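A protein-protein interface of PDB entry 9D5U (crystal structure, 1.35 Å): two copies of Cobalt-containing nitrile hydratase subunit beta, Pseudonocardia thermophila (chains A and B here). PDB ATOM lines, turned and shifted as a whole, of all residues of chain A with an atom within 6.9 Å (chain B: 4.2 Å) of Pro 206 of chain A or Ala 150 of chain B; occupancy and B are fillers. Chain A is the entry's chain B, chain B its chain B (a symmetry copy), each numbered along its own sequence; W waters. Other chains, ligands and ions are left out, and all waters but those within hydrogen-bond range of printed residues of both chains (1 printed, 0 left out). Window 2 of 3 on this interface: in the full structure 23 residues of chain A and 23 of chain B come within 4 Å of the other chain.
Of the 9 printed residues of chain A, 4 touch a printed residue of chain B. Hydrophobic or aromatic side chains of chain B that line the printed part of chain A: Ala 150 and Pro 152.
OG of Ser 148 of chain B is in hydrogen-bond range of N of Ala 150 of chain B (3.1 Å). The backbone carbonyl oxygen (O) of Gly 205 of chain A sits close to the side-chain amide oxygen (OE1) of Gln 201 of chain A (3.3 Å).
Among the printed residues, merely in contact across the chains: Glu 207 of chain A with Ala 150 of chain B, Pro 206 of chain A with Ala 150 of chain B, Trp 204 of chain A with Ala 150 of chain B and Gly 205 of chain A with Ala 150 of chain B.
O of Trp 204 of chain A sits at hydrogen-bond distance from OG of Ser 151 of chain B, at 2.8 Å. The backbone nitrogen of Pro 152 of chain B lies close to the side-chain carboxylate of Glu 207 of chain A (3.1 Å). N of Gly 205 of chain A lies within hydrogen-bond range of O of Thr 149 of chain B (3.3 Å). O of Trp 204 of chain A lies close to O of Thr 149 of chain B (3.2 Å). The backbone NH of Ser 151 of chain B lies within hydrogen-bond range of the side-chain carboxylate of Glu 207 of chain A (2.7 Å).
Water W1 bridges the backbone carbonyl oxygen (O) of Thr 149 of chain B (2.8 Å) and the backbone carbonyl oxygen (O) of Leu 203 of chain A (2.8 Å).
Printed residues of chain B within 4 Å of Trp 204 of chain A: Thr 149 (3.2 Å), Ala 150 (3.6 Å) and Ser 151 (2.8 Å). Of the printed residues of chain B, Gly 205 of chain A touches Thr 149 (3.3 Å) and Ala 150 (3.98 Å). Of chain B, only Ala 150 comes within 4 Å of Pro 206 of chain A. Asp 209 of chain A touches none of the printed residues of chain B. Of the printed residues of chain A, Thr 149 of chain B touches Trp 204 (3.2 Å) and Gly 205 (3.3 Å). Ala 150 of chain B touches just these residues of chain A: Trp 204, Gly 205, Pro 206 and Glu 207. Printed residues of chain A within 4 Å of Pro 152 of chain B: Glu 207 (3.1 Å). The nearest printed residue of chain B that does not touch Pro 206 of chain A is Thr 149 of chain B (4.5 Å). The nearest printed residue of chain B that does not touch Glu 207 of chain A is Thr 149 of chain B (5.1 Å).
No position is printed for both chains. Of the 9 pairs that touch across the chains among the printed residues, none has its exchanged pair printed and touching as well.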
ATOM      1  N   ALA A 200      19.335  16.519  -2.634  1.00  0.00           N
ATOM      2  CA  ALA A 200      18.905  15.467  -3.550  1.00  0.00           C
ATOM      3  C   ALA A 200      20.102  14.698  -4.113  1.00  0.00           C
ATOM      4  O   ALA A 200      19.992  13.508  -4.421  1.00  0.00           O
ATOM      5  CB  ALA A 200      18.005  16.038  -4.652  1.00  0.00           C
ATOM      6  N   GLN A 201      21.258  15.344  -4.250  1.00  0.00           N
ATOM      7  CA  GLN A 201      22.399  14.613  -4.794  1.00  0.00           C
ATOM      8  C   GLN A 201      22.982  13.655  -3.765  1.00  0.00           C
ATOM      9  O   GLN A 201      23.522  12.604  -4.134  1.00  0.00           O
ATOM     10  CB  GLN A 201      23.474  15.587  -5.266  1.00  0.00           C
ATOM     11  CG  GLN A 201      22.897  16.788  -5.993  1.00  0.00           C
ATOM     12  CD  GLN A 201      22.647  16.491  -7.427  1.00  0.00           C
ATOM     13  OE1 GLN A 201      21.880  15.578  -7.734  1.00  0.00           O
ATOM     14  NE2 GLN A 201      23.270  17.271  -8.334  1.00  0.00           N
ATOM     15  N   LEU A 203      20.993  12.096  -1.827  1.00  0.00           N
ATOM     16  CA  LEU A 203      19.997  11.031  -1.804  1.00  0.00           C
ATOM     17  C   LEU A 203      20.068  10.143  -3.046  1.00  0.00           C
ATOM     18  O   LEU A 203      20.061   8.908  -2.937  1.00  0.00           O
ATOM     19  CB  LEU A 203      18.607  11.620  -1.584  1.00  0.00           C
ATOM     20  CG  LEU A 203      18.463  12.347  -0.249  1.00  0.00           C
ATOM     21  CD1 LEU A 203      17.074  12.962  -0.136  1.00  0.00           C
ATOM     22  CD2 LEU A 203      18.728  11.413   0.929  1.00  0.00           C
ATOM     23  N   TRP A 204      20.157  10.738  -4.230  1.00  0.00           N
ATOM     24  CA  TRP A 204      19.896  10.023  -5.474  1.00  0.00           C
ATOM     25  C   TRP A 204      21.124   9.904  -6.359  1.00  0.00           C
ATOM     26  O   TRP A 204      21.025   9.367  -7.467  1.00  0.00           O
ATOM     27  CB  TRP A 204      18.731  10.698  -6.237  1.00  0.00           C
ATOM     28  CG  TRP A 204      17.591  11.087  -5.297  1.00  0.00           C
ATOM     29  CD1 TRP A 204      17.175  12.365  -4.965  1.00  0.00           C
ATOM     30  CD2 TRP A 204      16.731  10.193  -4.579  1.00  0.00           C
ATOM     31  NE1 TRP A 204      16.128  12.305  -4.075  1.00  0.00           N
ATOM     32  CE2 TRP A 204      15.833  10.991  -3.817  1.00  0.00           C
ATOM     33  CE3 TRP A 204      16.638   8.802  -4.500  1.00  0.00           C
ATOM     34  CZ2 TRP A 204      14.857  10.442  -2.989  1.00  0.00           C
ATOM     35  CZ3 TRP A 204      15.669   8.255  -3.669  1.00  0.00           C
ATOM     36  CH2 TRP A 204      14.783   9.080  -2.925  1.00  0.00           C
ATOM     37  N   GLY A 205      22.280  10.381  -5.906  1.00  0.00           N
ATOM     38  CA  GLY A 205      23.479  10.329  -6.707  1.00  0.00           C
ATOM     39  C   GLY A 205      23.500  11.431  -7.744  1.00  0.00           C
ATOM     40  O   GLY A 205      23.142  12.585  -7.481  1.00  0.00           O
ATOM     41  N   PRO A 206      23.922  11.085  -8.958  1.00  0.00           N
ATOM     42  CA  PRO A 206      23.831  12.044 -10.076  1.00  0.00           C
ATOM     43  C   PRO A 206      22.403  12.261 -10.576  1.00  0.00           C
ATOM     44  O   PRO A 206      22.152  13.283 -11.235  1.00  0.00           O
ATOM     45  CB  PRO A 206      24.675  11.379 -11.168  1.00  0.00           C
ATOM     46  CG  PRO A 206      24.544   9.879 -10.845  1.00  0.00           C
ATOM     47  CD  PRO A 206      24.516   9.793  -9.355  1.00  0.00           C
ATOM     48  N   GLU A 207      21.470  11.326 -10.306  1.00  0.00           N
ATOM     49  CA  GLU A 207      20.097  11.444 -10.786  1.00  0.00           C
ATOM     50  C   GLU A 207      19.278  12.458 -10.008  1.00  0.00           C
ATOM     51  O   GLU A 207      18.104  12.660 -10.344  1.00  0.00           O
ATOM     52  CB  GLU A 207      19.376  10.092 -10.752  1.00  0.00           C
ATOM     53  CG  GLU A 207      19.714   9.128 -11.885  1.00  0.00           C
ATOM     54  CD  GLU A 207      21.035   8.401 -11.694  1.00  0.00           C
ATOM     55  OE1 GLU A 207      21.674   8.578 -10.633  1.00  0.00           O
ATOM     56  OE2 GLU A 207      21.390   7.596 -12.596  1.00  0.00           O
ATOM     57  N   GLY A 208      19.860  13.097  -8.985  1.00  0.00           N
ATOM     58  CA  GLY A 208      19.124  14.055  -8.162  1.00  0.00           C
ATOM     59  C   GLY A 208      19.153  15.484  -8.702  1.00  0.00           C
ATOM     60  O   GLY A 208      20.084  15.902  -9.381  1.00  0.00           O
ATOM     61  N   ASP A 209      18.125  16.243  -8.382  1.00  0.00           N
ATOM     62  CA  ASP A 209      18.089  17.688  -8.916  1.00  0.00           C
ATOM     63  C   ASP A 209      19.244  18.691  -8.397  1.00  0.00           C
ATOM     64  O   ASP A 209      19.241  18.544  -7.044  1.00  0.00           O
ATOM     65  CB  ASP A 209      16.649  18.151  -8.452  1.00  0.00           C
ATOM     66  CG  ASP A 209      16.342  19.512  -9.028  1.00  0.00           C
ATOM     67  OD1 ASP A 209      17.099  20.453  -8.702  1.00  0.00           O
ATOM     68  OD2 ASP A 209      15.367  19.642  -9.812  1.00  0.00           O
ATOM     69  N   SER B 148      28.200   2.720  -6.097  1.00  0.00           N
ATOM     70  CA  SER B 148      27.637   3.976  -6.567  1.00  0.00           C
ATOM     71  C   SER B 148      26.307   4.282  -5.874  1.00  0.00           C
ATOM     72  O   SER B 148      25.522   3.382  -5.537  1.00  0.00           O
ATOM     73  CB  SER B 148      27.436   3.892  -8.089  1.00  0.00           C
ATOM     74  OG  SER B 148      26.739   5.004  -8.596  1.00  0.00           O
ATOM     75  N   THR B 149      26.056   5.578  -5.657  1.00  0.00           N
ATOM     76  CA  THR B 149      24.772   6.044  -5.141  1.00  0.00           C
ATOM     77  C   THR B 149      23.835   6.559  -6.243  1.00  0.00           C
ATOM     78  O   THR B 149      22.764   7.105  -5.927  1.00  0.00           O
ATOM     79  CB  THR B 149      24.993   7.113  -4.079  1.00  0.00           C
ATOM     80  OG1 THR B 149      25.766   8.181  -4.645  1.00  0.00           O
ATOM     81  CG2 THR B 149      25.742   6.518  -2.886  1.00  0.00           C
ATOM     82  N   ALA B 150      24.208   6.406  -7.518  1.00  0.00           N
ATOM     83  CA  ALA B 150      23.324   6.829  -8.595  1.00  0.00           C
ATOM     84  C   ALA B 150      22.079   5.954  -8.600  1.00  0.00           C
ATOM     85  O   ALA B 150      22.100   4.795  -8.174  1.00  0.00           O
ATOM     86  CB  ALA B 150      24.018   6.744  -9.938  1.00  0.00           C
ATOM     87  N   SER B 151      20.979   6.528  -9.080  1.00  0.00           N
ATOM     88  CA  SER B 151      19.664   5.892  -8.996  1.00  0.00           C
ATOM     89  C   SER B 151      18.958   6.029 -10.334  1.00  0.00           C
ATOM     90  O   SER B 151      17.911   6.680 -10.451  1.00  0.00           O
ATOM     91  CB  SER B 151      18.853   6.514  -7.865  1.00  0.00           C
ATOM     92  OG  SER B 151      18.738   7.915  -8.063  1.00  0.00           O
ATOM     93  N   PRO B 152      19.508   5.410 -11.370  1.00  0.00           N
ATOM     94  CA  PRO B 152      18.949   5.583 -12.717  1.00  0.00           C
ATOM     95  C   PRO B 152      17.513   5.077 -12.817  1.00  0.00           C
ATOM     96  O   PRO B 152      17.089   4.172 -12.095  1.00  0.00           O
ATOM     97  CB  PRO B 152      19.895   4.760 -13.593  1.00  0.00           C
ATOM     98  CG  PRO B 152      20.429   3.716 -12.631  1.00  0.00           C
ATOM     99  CD  PRO B 152      20.650   4.494 -11.371  1.00  0.00           C
ATOM    100  N   ARG B 163      23.783   0.025  -2.474  1.00  0.00           N
ATOM    101  CA  ARG B 163      24.238   1.328  -2.937  1.00  0.00           C
ATOM    102  C   ARG B 163      24.868   2.131  -1.808  1.00  0.00           C
ATOM    103  O   ARG B 163      24.370   2.162  -0.676  1.00  0.00           O
ATOM    104  CB  ARG B 163      23.068   2.102  -3.506  1.00  0.00           C
ATOM    105  CG  ARG B 163      22.451   1.428  -4.693  1.00  0.00           C
ATOM    106  CD  ARG B 163      21.470   2.378  -5.320  1.00  0.00           C
ATOM    107  NE  ARG B 163      20.586   1.707  -6.251  1.00  0.00           N
ATOM    108  CZ  ARG B 163      19.465   2.240  -6.706  1.00  0.00           C
ATOM    109  NH1 ARG B 163      19.077   3.453  -6.323  1.00  0.00           N
ATOM    110  NH2 ARG B 163      18.712   1.534  -7.555  1.00  0.00           N
HETATM  111  O   HOH W   1      20.474   6.591  -4.480  1.00  0.00           O
